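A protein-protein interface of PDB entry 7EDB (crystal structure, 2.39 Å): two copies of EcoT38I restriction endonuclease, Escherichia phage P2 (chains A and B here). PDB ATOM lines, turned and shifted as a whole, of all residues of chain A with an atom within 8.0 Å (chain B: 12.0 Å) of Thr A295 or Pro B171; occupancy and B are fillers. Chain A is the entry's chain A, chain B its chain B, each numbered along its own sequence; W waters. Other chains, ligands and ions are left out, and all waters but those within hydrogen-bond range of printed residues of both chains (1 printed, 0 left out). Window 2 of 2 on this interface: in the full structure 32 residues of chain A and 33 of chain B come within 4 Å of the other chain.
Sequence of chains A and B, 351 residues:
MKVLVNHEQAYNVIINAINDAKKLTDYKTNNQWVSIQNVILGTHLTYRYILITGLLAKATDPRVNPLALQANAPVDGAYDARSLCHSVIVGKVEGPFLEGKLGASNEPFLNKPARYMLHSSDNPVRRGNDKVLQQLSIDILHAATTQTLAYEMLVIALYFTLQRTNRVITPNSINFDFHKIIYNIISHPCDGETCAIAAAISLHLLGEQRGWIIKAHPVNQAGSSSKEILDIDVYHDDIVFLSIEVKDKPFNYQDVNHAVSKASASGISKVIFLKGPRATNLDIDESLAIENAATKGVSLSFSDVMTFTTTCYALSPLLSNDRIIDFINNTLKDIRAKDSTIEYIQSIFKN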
ATOM      1  N   VAL A 260     -21.951  -2.162  19.419  1.00  0.00           N
ATOM      2  CA  VAL A 260     -22.768  -3.012  18.569  1.00  0.00           C
ATOM      3  C   VAL A 260     -23.445  -4.105  19.392  1.00  0.00           C
ATOM      4  O   VAL A 260     -24.623  -4.433  19.182  1.00  0.00           O
ATOM      5  CB  VAL A 260     -21.894  -3.619  17.454  1.00  0.00           C
ATOM      6  CG1 VAL A 260     -22.589  -4.838  16.825  1.00  0.00           C
ATOM      7  CG2 VAL A 260     -21.546  -2.568  16.405  1.00  0.00           C
ATOM      8  N   SER A 261     -22.705  -4.701  20.330  1.00  0.00           N
ATOM      9  CA  SER A 261     -23.266  -5.801  21.103  1.00  0.00           C
ATOM     10  C   SER A 261     -24.403  -5.321  21.991  1.00  0.00           C
ATOM     11  O   SER A 261     -25.415  -6.015  22.138  1.00  0.00           O
ATOM     12  CB  SER A 261     -22.167  -6.481  21.926  1.00  0.00           C
ATOM     13  OG  SER A 261     -21.243  -7.147  21.056  1.00  0.00           O
ATOM     14  N   ALA A 263     -26.413  -2.794  21.324  1.00  0.00           N
ATOM     15  CA  ALA A 263     -27.558  -2.606  20.435  1.00  0.00           C
ATOM     16  C   ALA A 263     -28.152  -3.942  20.008  1.00  0.00           C
ATOM     17  O   ALA A 263     -29.379  -4.085  19.917  1.00  0.00           O
ATOM     18  CB  ALA A 263     -27.148  -1.803  19.203  1.00  0.00           C
ATOM     19  N   SER A 264     -27.295  -4.918  19.717  1.00  0.00           N
ATOM     20  CA  SER A 264     -27.777  -6.228  19.300  1.00  0.00           C
ATOM     21  C   SER A 264     -28.595  -6.902  20.403  1.00  0.00           C
ATOM     22  O   SER A 264     -29.652  -7.483  20.133  1.00  0.00           O
ATOM     23  CB  SER A 264     -26.592  -7.100  18.893  1.00  0.00           C
ATOM     24  OG  SER A 264     -27.056  -8.335  18.393  1.00  0.00           O
ATOM     25  N   ALA A 265     -28.132  -6.820  21.652  1.00  0.00           N
ATOM     26  CA  ALA A 265     -28.843  -7.454  22.756  1.00  0.00           C
ATOM     27  C   ALA A 265     -30.190  -6.798  23.039  1.00  0.00           C
ATOM     28  O   ALA A 265     -31.060  -7.443  23.630  1.00  0.00           O
ATOM     29  CB  ALA A 265     -27.975  -7.449  24.022  1.00  0.00           C
ATOM     30  N   SER A 266     -30.393  -5.548  22.632  1.00  0.00           N
ATOM     31  CA  SER A 266     -31.682  -4.885  22.814  1.00  0.00           C
ATOM     32  C   SER A 266     -32.544  -4.887  21.552  1.00  0.00           C
ATOM     33  O   SER A 266     -33.625  -4.290  21.559  1.00  0.00           O
ATOM     34  CB  SER A 266     -31.479  -3.439  23.287  1.00  0.00           C
ATOM     35  OG  SER A 266     -30.650  -3.377  24.432  1.00  0.00           O
ATOM     36  N   GLY A 267     -32.090  -5.525  20.468  1.00  0.00           N
ATOM     37  CA  GLY A 267     -32.854  -5.561  19.235  1.00  0.00           C
ATOM     38  C   GLY A 267     -32.901  -4.267  18.436  1.00  0.00           C
ATOM     39  O   GLY A 267     -33.825  -4.083  17.639  1.00  0.00           O
ATOM     40  N   LEU A 288     -14.759  -3.921   8.071  1.00  0.00           N
ATOM     41  CA  LEU A 288     -14.783  -5.158   8.845  1.00  0.00           C
ATOM     42  C   LEU A 288     -15.677  -5.022  10.073  1.00  0.00           C
ATOM     43  O   LEU A 288     -16.446  -5.942  10.394  1.00  0.00           O
ATOM     44  CB  LEU A 288     -13.359  -5.551   9.245  1.00  0.00           C
ATOM     45  CG  LEU A 288     -13.144  -6.840  10.051  1.00  0.00           C
ATOM     46  CD1 LEU A 288     -13.558  -8.089   9.268  1.00  0.00           C
ATOM     47  CD2 LEU A 288     -11.698  -6.942  10.510  1.00  0.00           C
ATOM     48  N   ALA A 289     -15.592  -3.881  10.770  1.00  0.00           N
ATOM     49  CA  ALA A 289     -16.506  -3.614  11.878  1.00  0.00           C
ATOM     50  C   ALA A 289     -17.954  -3.666  11.417  1.00  0.00           C
ATOM     51  O   ALA A 289     -18.810  -4.248  12.096  1.00  0.00           O
ATOM     52  CB  ALA A 289     -16.205  -2.258  12.513  1.00  0.00           C
ATOM     53  N   ILE A 290     -18.240  -3.073  10.254  1.00  0.00           N
ATOM     54  CA  ILE A 290     -19.605  -3.019   9.738  1.00  0.00           C
ATOM     55  C   ILE A 290     -20.078  -4.412   9.334  1.00  0.00           C
ATOM     56  O   ILE A 290     -21.220  -4.804   9.614  1.00  0.00           O
ATOM     57  CB  ILE A 290     -19.681  -2.017   8.568  1.00  0.00           C
ATOM     58  CG1 ILE A 290     -19.544  -0.580   9.079  1.00  0.00           C
ATOM     59  CG2 ILE A 290     -20.962  -2.191   7.772  1.00  0.00           C
ATOM     60  CD1 ILE A 290     -19.254   0.461   7.974  1.00  0.00           C
ATOM     61  N   GLU A 291     -19.203  -5.184   8.684  1.00  0.00           N
ATOM     62  CA  GLU A 291     -19.503  -6.581   8.385  1.00  0.00           C
ATOM     63  C   GLU A 291     -19.787  -7.370   9.663  1.00  0.00           C
ATOM     64  O   GLU A 291     -20.780  -8.106   9.740  1.00  0.00           O
ATOM     65  CB  GLU A 291     -18.341  -7.206   7.603  1.00  0.00           C
ATOM     66  CG  GLU A 291     -18.523  -7.180   6.078  1.00  0.00           C
ATOM     67  CD  GLU A 291     -17.279  -6.705   5.299  1.00  0.00           C
ATOM     68  OE1 GLU A 291     -17.443  -5.936   4.314  1.00  0.00           O
ATOM     69  OE2 GLU A 291     -16.144  -7.098   5.663  1.00  0.00           O
ATOM     70  N   ASN A 292     -18.928  -7.226  10.682  1.00  0.00           N
ATOM     71  CA  ASN A 292     -19.149  -7.927  11.948  1.00  0.00           C
ATOM     72  C   ASN A 292     -20.505  -7.560  12.541  1.00  0.00           C
ATOM     73  O   ASN A 292     -21.275  -8.442  12.944  1.00  0.00           O
ATOM     74  CB  ASN A 292     -18.016  -7.618  12.934  1.00  0.00           C
ATOM     75  CG  ASN A 292     -18.311  -8.105  14.370  1.00  0.00           C
ATOM     76  OD1 ASN A 292     -18.642  -7.301  15.271  1.00  0.00           O
ATOM     77  ND2 ASN A 292     -18.179  -9.420  14.590  1.00  0.00           N
ATOM     78  N   ALA A 293     -20.829  -6.258  12.566  1.00  0.00           N
ATOM     79  CA  ALA A 293     -22.121  -5.821  13.092  1.00  0.00           C
ATOM     80  C   ALA A 293     -23.273  -6.440  12.311  1.00  0.00           C
ATOM     81  O   ALA A 293     -24.283  -6.845  12.900  1.00  0.00           O
ATOM     82  CB  ALA A 293     -22.228  -4.293  13.061  1.00  0.00           C
ATOM     83  N   ALA A 294     -23.143  -6.503  10.981  1.00  0.00           N
ATOM     84  CA  ALA A 294     -24.214  -7.043  10.147  1.00  0.00           C
ATOM     85  C   ALA A 294     -24.578  -8.469  10.556  1.00  0.00           C
ATOM     86  O   ALA A 294     -25.766  -8.816  10.620  1.00  0.00           O
ATOM     87  CB  ALA A 294     -23.810  -6.992   8.675  1.00  0.00           C
ATOM     88  N   THR A 295     -23.573  -9.308  10.847  1.00  0.00           N
ATOM     89  CA  THR A 295     -23.881 -10.669  11.284  1.00  0.00           C
ATOM     90  C   THR A 295     -24.573 -10.669  12.645  1.00  0.00           C
ATOM     91  O   THR A 295     -25.364 -11.568  12.939  1.00  0.00           O
ATOM     92  CB  THR A 295     -22.619 -11.536  11.338  1.00  0.00           C
ATOM     93  OG1 THR A 295     -21.895 -11.261  12.542  1.00  0.00           O
ATOM     94  CG2 THR A 295     -21.718 -11.283  10.139  1.00  0.00           C
ATOM     95  N   LYS A 296     -24.311  -9.670  13.477  1.00  0.00           N
ATOM     96  CA  LYS A 296     -24.997  -9.566  14.756  1.00  0.00           C
ATOM     97  C   LYS A 296     -26.351  -8.875  14.647  1.00  0.00           C
ATOM     98  O   LYS A 296     -26.932  -8.530  15.681  1.00  0.00           O
ATOM     99  CB  LYS A 296     -24.108  -8.841  15.769  1.00  0.00           C
ATOM    100  CG  LYS A 296     -22.858  -9.642  16.107  1.00  0.00           C
ATOM    101  CD  LYS A 296     -22.003  -8.968  17.162  1.00  0.00           C
ATOM    102  CE  LYS A 296     -20.857  -9.901  17.575  1.00  0.00           C
ATOM    103  NZ  LYS A 296     -20.227  -9.496  18.877  1.00  0.00           N
ATOM    104  N   GLY A 297     -26.864  -8.673  13.431  1.00  0.00           N
ATOM    105  CA  GLY A 297     -28.159  -8.047  13.245  1.00  0.00           C
ATOM    106  C   GLY A 297     -28.178  -6.547  13.398  1.00  0.00           C
ATOM    107  O   GLY A 297     -29.252  -5.968  13.585  1.00  0.00           O
ATOM    108  N   VAL A 298     -27.023  -5.892  13.323  1.00  0.00           N
ATOM    109  CA  VAL A 298     -26.946  -4.444  13.454  1.00  0.00           C
ATOM    110  C   VAL A 298     -26.411  -3.840  12.165  1.00  0.00           C
ATOM    111  O   VAL A 298     -25.323  -4.202  11.697  1.00  0.00           O
ATOM    112  CB  VAL A 298     -26.066  -4.018  14.639  1.00  0.00           C
ATOM    113  CG1 VAL A 298     -25.797  -2.500  14.553  1.00  0.00           C
ATOM    114  CG2 VAL A 298     -26.749  -4.384  15.948  1.00  0.00           C
ATOM    115  N   SER A 299     -27.163  -2.899  11.613  1.00  0.00           N
ATOM    116  CA  SER A 299     -26.660  -2.050  10.544  1.00  0.00           C
ATOM    117  C   SER A 299     -25.864  -0.901  11.169  1.00  0.00           C
ATOM    118  O   SER A 299     -26.433  -0.014  11.820  1.00  0.00           O
ATOM    119  CB  SER A 299     -27.822  -1.551   9.695  1.00  0.00           C
ATOM    120  OG  SER A 299     -27.377  -0.589   8.758  1.00  0.00           O
ATOM    121  N   ASN B 166     -20.493 -17.901  28.286  1.00  0.00           N
ATOM    122  CA  ASN B 166     -20.862 -16.509  27.999  1.00  0.00           C
ATOM    123  C   ASN B 166     -22.126 -16.546  27.150  1.00  0.00           C
ATOM    124  O   ASN B 166     -22.086 -16.377  25.928  1.00  0.00           O
ATOM    125  CB  ASN B 166     -19.705 -15.702  27.291  1.00  0.00           C
ATOM    126  CG  ASN B 166     -20.086 -14.241  27.003  1.00  0.00           C
ATOM    127  OD1 ASN B 166     -20.303 -13.438  27.922  1.00  0.00           O
ATOM    128  ND2 ASN B 166     -20.136 -13.891  25.722  1.00  0.00           N
ATOM    129  N   ARG B 167     -23.259 -16.751  27.818  1.00  0.00           N
ATOM    130  CA  ARG B 167     -24.546 -16.955  27.163  1.00  0.00           C
ATOM    131  C   ARG B 167     -25.052 -15.691  26.483  1.00  0.00           C
ATOM    132  O   ARG B 167     -25.856 -14.954  27.061  1.00  0.00           O
ATOM    133  CB  ARG B 167     -25.586 -17.454  28.175  1.00  0.00           C
ATOM    134  CG  ARG B 167     -25.018 -18.295  29.330  1.00  0.00           C
ATOM    135  CD  ARG B 167     -24.687 -17.443  30.564  1.00  0.00           C
ATOM    136  NE  ARG B 167     -25.893 -16.887  31.175  1.00  0.00           N
ATOM    137  CZ  ARG B 167     -25.895 -15.944  32.113  1.00  0.00           C
ATOM    138  NH1 ARG B 167     -24.750 -15.437  32.553  1.00  0.00           N
ATOM    139  NH2 ARG B 167     -27.046 -15.503  32.606  1.00  0.00           N
ATOM    140  N   VAL B 168     -24.589 -15.429  25.263  1.00  0.00           N
ATOM    141  CA  VAL B 168     -25.177 -14.409  24.401  1.00  0.00           C
ATOM    142  C   VAL B 168     -25.769 -15.113  23.187  1.00  0.00           C
ATOM    143  O   VAL B 168     -25.125 -15.988  22.595  1.00  0.00           O
ATOM    144  CB  VAL B 168     -24.155 -13.325  23.992  1.00  0.00           C
ATOM    145  CG1 VAL B 168     -23.490 -12.714  25.229  1.00  0.00           C
ATOM    146  CG2 VAL B 168     -23.099 -13.863  23.021  1.00  0.00           C
ATOM    147  N   ILE B 169     -27.003 -14.771  22.840  1.00  0.00           N
ATOM    148  CA  ILE B 169     -27.687 -15.433  21.732  1.00  0.00           C
ATOM    149  C   ILE B 169     -27.353 -14.703  20.441  1.00  0.00           C
ATOM    150  O   ILE B 169     -27.536 -13.485  20.342  1.00  0.00           O
ATOM    151  CB  ILE B 169     -29.208 -15.496  21.962  1.00  0.00           C
ATOM    152  CG1 ILE B 169     -29.554 -16.577  23.001  1.00  0.00           C
ATOM    153  CG2 ILE B 169     -29.947 -15.732  20.635  1.00  0.00           C
ATOM    154  CD1 ILE B 169     -29.268 -18.009  22.558  1.00  0.00           C
ATOM    155  N   THR B 170     -26.856 -15.451  19.458  1.00  0.00           N
ATOM    156  CA  THR B 170     -26.449 -14.937  18.152  1.00  0.00           C
ATOM    157  C   THR B 170     -27.668 -14.568  17.326  1.00  0.00           C
ATOM    158  O   THR B 170     -28.380 -15.470  16.866  1.00  0.00           O
ATOM    159  CB  THR B 170     -25.620 -15.980  17.404  1.00  0.00           C
ATOM    160  OG1 THR B 170     -26.333 -17.227  17.379  1.00  0.00           O
ATOM    161  CG2 THR B 170     -24.262 -16.174  18.073  1.00  0.00           C
ATOM    162  N   PRO B 171     -27.952 -13.287  17.107  1.00  0.00           N
ATOM    163  CA  PRO B 171     -29.128 -12.933  16.309  1.00  0.00           C
ATOM    164  C   PRO B 171     -28.962 -13.388  14.868  1.00  0.00           C
ATOM    165  O   PRO B 171     -27.906 -13.856  14.428  1.00  0.00           O
ATOM    166  CB  PRO B 171     -29.193 -11.400  16.402  1.00  0.00           C
ATOM    167  CG  PRO B 171     -28.301 -11.039  17.542  1.00  0.00           C
ATOM    168  CD  PRO B 171     -27.229 -12.090  17.569  1.00  0.00           C
ATOM    169  N   ASN B 172     -30.056 -13.290  14.134  1.00  0.00           N
ATOM    170  CA  ASN B 172     -29.925 -13.468  12.706  1.00  0.00           C
ATOM    171  C   ASN B 172     -29.222 -12.252  12.097  1.00  0.00           C
ATOM    172  O   ASN B 172     -29.109 -11.179  12.699  1.00  0.00           O
ATOM    173  CB  ASN B 172     -31.293 -13.727  12.060  1.00  0.00           C
ATOM    174  CG  ASN B 172     -31.610 -15.237  11.915  1.00  0.00           C
ATOM    175  OD1 ASN B 172     -30.860 -16.098  12.382  1.00  0.00           O
ATOM    176  ND2 ASN B 172     -32.724 -15.546  11.267  1.00  0.00           N
ATOM    177  N   SER B 173     -28.665 -12.474  10.910  1.00  0.00           N
ATOM    178  CA  SER B 173     -28.018 -11.409  10.165  1.00  0.00           C
ATOM    179  C   SER B 173     -29.047 -10.348   9.809  1.00  0.00           C
ATOM    180  O   SER B 173     -30.249 -10.620   9.705  1.00  0.00           O
ATOM    181  CB  SER B 173     -27.387 -11.937   8.872  1.00  0.00           C
ATOM    182  OG  SER B 173     -26.226 -12.717   9.107  1.00  0.00           O
ATOM    183  N   ILE B 174     -28.558  -9.125   9.599  1.00  0.00           N
ATOM    184  CA  ILE B 174     -29.442  -8.048   9.169  1.00  0.00           C
ATOM    185  C   ILE B 174     -30.116  -8.447   7.854  1.00  0.00           C
ATOM    186  O   ILE B 174     -29.488  -9.039   6.963  1.00  0.00           O
ATOM    187  CB  ILE B 174     -28.653  -6.725   9.086  1.00  0.00           C
ATOM    188  CG1 ILE B 174     -29.602  -5.526   8.995  1.00  0.00           C
ATOM    189  CG2 ILE B 174     -27.642  -6.720   7.929  1.00  0.00           C
ATOM    190  CD1 ILE B 174     -30.312  -5.208  10.302  1.00  0.00           C
ATOM    191  N   ASN B 175     -31.430  -8.205   7.761  1.00  0.00           N
ATOM    192  CA  ASN B 175     -32.153  -8.499   6.522  1.00  0.00           C
ATOM    193  C   ASN B 175     -31.601  -7.686   5.359  1.00  0.00           C
ATOM    194  O   ASN B 175     -31.367  -8.214   4.263  1.00  0.00           O
ATOM    195  CB  ASN B 175     -33.645  -8.200   6.682  1.00  0.00           C
ATOM    196  CG  ASN B 175     -34.362  -9.208   7.552  1.00  0.00           C
ATOM    197  OD1 ASN B 175     -33.746  -9.978   8.285  1.00  0.00           O
ATOM    198  ND2 ASN B 175     -35.684  -9.197   7.480  1.00  0.00           N
ATOM    199  N   PHE B 176     -31.388  -6.391   5.584  1.00  0.00           N
ATOM    200  CA  PHE B 176     -31.043  -5.440   4.537  1.00  0.00           C
ATOM    201  C   PHE B 176     -29.690  -4.817   4.867  1.00  0.00           C
ATOM    202  O   PHE B 176     -29.580  -4.025   5.809  1.00  0.00           O
ATOM    203  CB  PHE B 176     -32.136  -4.384   4.418  1.00  0.00           C
ATOM    204  CG  PHE B 176     -32.085  -3.596   3.147  1.00  0.00           C
ATOM    205  CD1 PHE B 176     -32.389  -4.193   1.938  1.00  0.00           C
ATOM    206  CD2 PHE B 176     -31.756  -2.253   3.163  1.00  0.00           C
ATOM    207  CE1 PHE B 176     -32.354  -3.470   0.763  1.00  0.00           C
ATOM    208  CE2 PHE B 176     -31.722  -1.518   1.986  1.00  0.00           C
ATOM    209  CZ  PHE B 176     -32.025  -2.129   0.787  1.00  0.00           C
ATOM    210  N   ASP B 177     -28.665  -5.177   4.093  1.00  0.00           N
ATOM    211  CA  ASP B 177     -27.298  -4.674   4.274  1.00  0.00           C
ATOM    212  C   ASP B 177     -27.088  -3.515   3.296  1.00  0.00           C
ATOM    213  O   ASP B 177     -26.578  -3.691   2.189  1.00  0.00           O
ATOM    214  CB  ASP B 177     -26.277  -5.797   4.063  1.00  0.00           C
ATOM    215  CG  ASP B 177     -24.862  -5.424   4.547  1.00  0.00           C
ATOM    216  OD1 ASP B 177     -24.514  -4.220   4.651  1.00  0.00           O
ATOM    217  OD2 ASP B 177     -24.077  -6.353   4.813  1.00  0.00           O
ATOM    218  N   PHE B 178     -27.478  -2.310   3.723  1.00  0.00           N
ATOM    219  CA  PHE B 178     -27.336  -1.143   2.859  1.00  0.00           C
ATOM    220  C   PHE B 178     -25.875  -0.864   2.539  1.00  0.00           C
ATOM    221  O   PHE B 178     -25.537  -0.565   1.389  1.00  0.00           O
ATOM    222  CB  PHE B 178     -27.978   0.080   3.503  1.00  0.00           C
ATOM    223  CG  PHE B 178     -27.996   1.289   2.611  1.00  0.00           C
ATOM    224  CD1 PHE B 178     -28.727   1.281   1.429  1.00  0.00           C
ATOM    225  CD2 PHE B 178     -27.283   2.430   2.947  1.00  0.00           C
ATOM    226  CE1 PHE B 178     -28.753   2.394   0.598  1.00  0.00           C
ATOM    227  CE2 PHE B 178     -27.312   3.558   2.131  1.00  0.00           C
ATOM    228  CZ  PHE B 178     -28.050   3.542   0.954  1.00  0.00           C
ATOM    229  N   HIS B 179     -24.991  -0.966   3.538  1.00  0.00           N
ATOM    230  CA  HIS B 179     -23.577  -0.690   3.301  1.00  0.00           C
ATOM    231  C   HIS B 179     -23.028  -1.539   2.166  1.00  0.00           C
ATOM    232  O   HIS B 179     -22.224  -1.061   1.356  1.00  0.00           O
ATOM    233  CB  HIS B 179     -22.758  -0.935   4.566  1.00  0.00           C
ATOM    234  CG  HIS B 179     -21.280  -0.863   4.335  1.00  0.00           C
ATOM    235  ND1 HIS B 179     -20.594   0.331   4.256  1.00  0.00           N
ATOM    236  CD2 HIS B 179     -20.363  -1.837   4.132  1.00  0.00           C
ATOM    237  CE1 HIS B 179     -19.314   0.090   4.032  1.00  0.00           C
ATOM    238  NE2 HIS B 179     -19.147  -1.218   3.952  1.00  0.00           N
ATOM    239  N   LYS B 180     -23.447  -2.804   2.097  1.00  0.00           N
ATOM    240  CA  LYS B 180     -23.009  -3.688   1.021  1.00  0.00           C
ATOM    241  C   LYS B 180     -23.516  -3.196  -0.331  1.00  0.00           C
ATOM    242  O   LYS B 180     -22.753  -3.116  -1.300  1.00  0.00           O
ATOM    243  CB  LYS B 180     -23.486  -5.119   1.309  1.00  0.00           C
ATOM    244  CG  LYS B 180     -23.374  -6.106   0.154  1.00  0.00           C
ATOM    245  CD  LYS B 180     -23.597  -7.545   0.649  1.00  0.00           C
ATOM    246  CE  LYS B 180     -25.010  -7.766   1.214  1.00  0.00           C
ATOM    247  NZ  LYS B 180     -25.150  -9.057   1.999  1.00  0.00           N
HETATM  248  O   HOH W   1     -26.604  -1.495   6.472  1.00  0.00           O
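No position is printed for both chains.
Of the 11 pairs that touch across the chains among the printed residues, none has its exchanged pair printed and touching as well.
OG of Ser A261 is in hydrogen-bond range of NZ of Lys A296.
The side-chain hydroxyl (OG) of Ser A264 is in hydrogen-bond range of the backbone carbonyl oxygen (O) of Lys A296 (2.7 Å).
The backbone carbonyl oxygen (O) of Asn A292 sits at hydrogen-bond distance from the side-chain hydroxyl (OG1) of Thr A295 (2.9 Å).
The backbone NH (N) of His B179 lies close to the side-chain carboxylate (OD1) of Asp B177, 3.5 Å away.
The backbone NH of Lys B180 is in hydrogen-bond range of the side-chain carboxylate of Asp B177, 3.1 Å away.
Water W1 lies within hydrogen-bond range of the side-chain hydroxyl (OG) of Ser A299 (2.6 Å), the backbone NH (N) of Phe B178 (3.0 Å) and the backbone NH (N) of His B179 (3.4 Å).
Of the printed residues of chain B, Thr A295 touches Pro B171 (3.7 Å), Asn B172 (3.8 Å) and Ser B173 (3.8 Å).
Pro B171 touches just these residues of chain A: Ser A264 (3.1 Å), Thr A295 (3.7 Å) and Lys A296 (3.4 Å).
Ser A264 touches just one residue of chain B: Pro B171.
No residue of chain B comes within 4 Å of Asn A292.
No residue of chain B comes within 4 Å of Ala A293.
Of chain B, only Ser B173 (3.5 Å), Ile B174 (3.0 Å) and Asp B177 (3.9 Å) come within 4 Å of Ala A294.
Of chain B, only Pro B171 (3.4 Å) comes within 4 Å of Lys A296.
Of the printed residues of chain A, Ile B174 touches Ala A294 (3.0 Å) and Gly A297 (3.5 Å).
Printed residues of chain A within 4 Å of Asp B177: Ala A294.
Printed residues of chain B within 4 Å of Gly A297: Asn B172 (3.3 Å) and Ile B174 (3.5 Å).
Printed residues of chain A within 4 Å of Ser B173: Ala A294 and Thr A295.
Printed residues of chain A within 4 Å of Asn B172: Thr A295 and Gly A297.
Ser A299 touches none of the printed residues of chain B.
Asn B175 touches none of the printed residues of chain A.
The nearest printed residue of chain A that does not touch Ile B174 is Ser A299 (4.1 Å).
O of Ala A294 is in hydrogen-bond range of N of Ile B174 (3.0 Å).
O of Asn B172 lies close to N of Gly A297 (3.4 Å).
Pro B171 touches Ser A264 (CG to OG, 3.1 Å).
CG of His B179 touches CG2 of Ile A290 (3.7 Å).
O of Ala A294 touches CA of Ser B173, at 3.5 Å.
OD2 of Asp B177 touches CB of Ala A294 (3.9 Å).
Thr A295 touches Pro B171.
Thr A295 touches Asn B172 (O to O, 3.8 Å).
Thr A295 touches Ser B173.
CG of Pro B171 touches O of Lys A296, at 3.4 Å.
Gly A297 touches Ile B174 (O to CD1, 3.5 Å).
Printed residues of chain A that touch a printed residue of chain B: Ser A264, Ile A290, Ala A294, Thr A295, Lys A296 and Gly A297.
Of the 15 printed residues of chain B, 6 touch a printed residue of chain A.
Hydrophobic or aromatic side chains of chain B within 4 Å of the printed part of chain A: Pro B171, Ile B174 and His B179.
Among the printed residues, 11 pairs touch across the chains.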
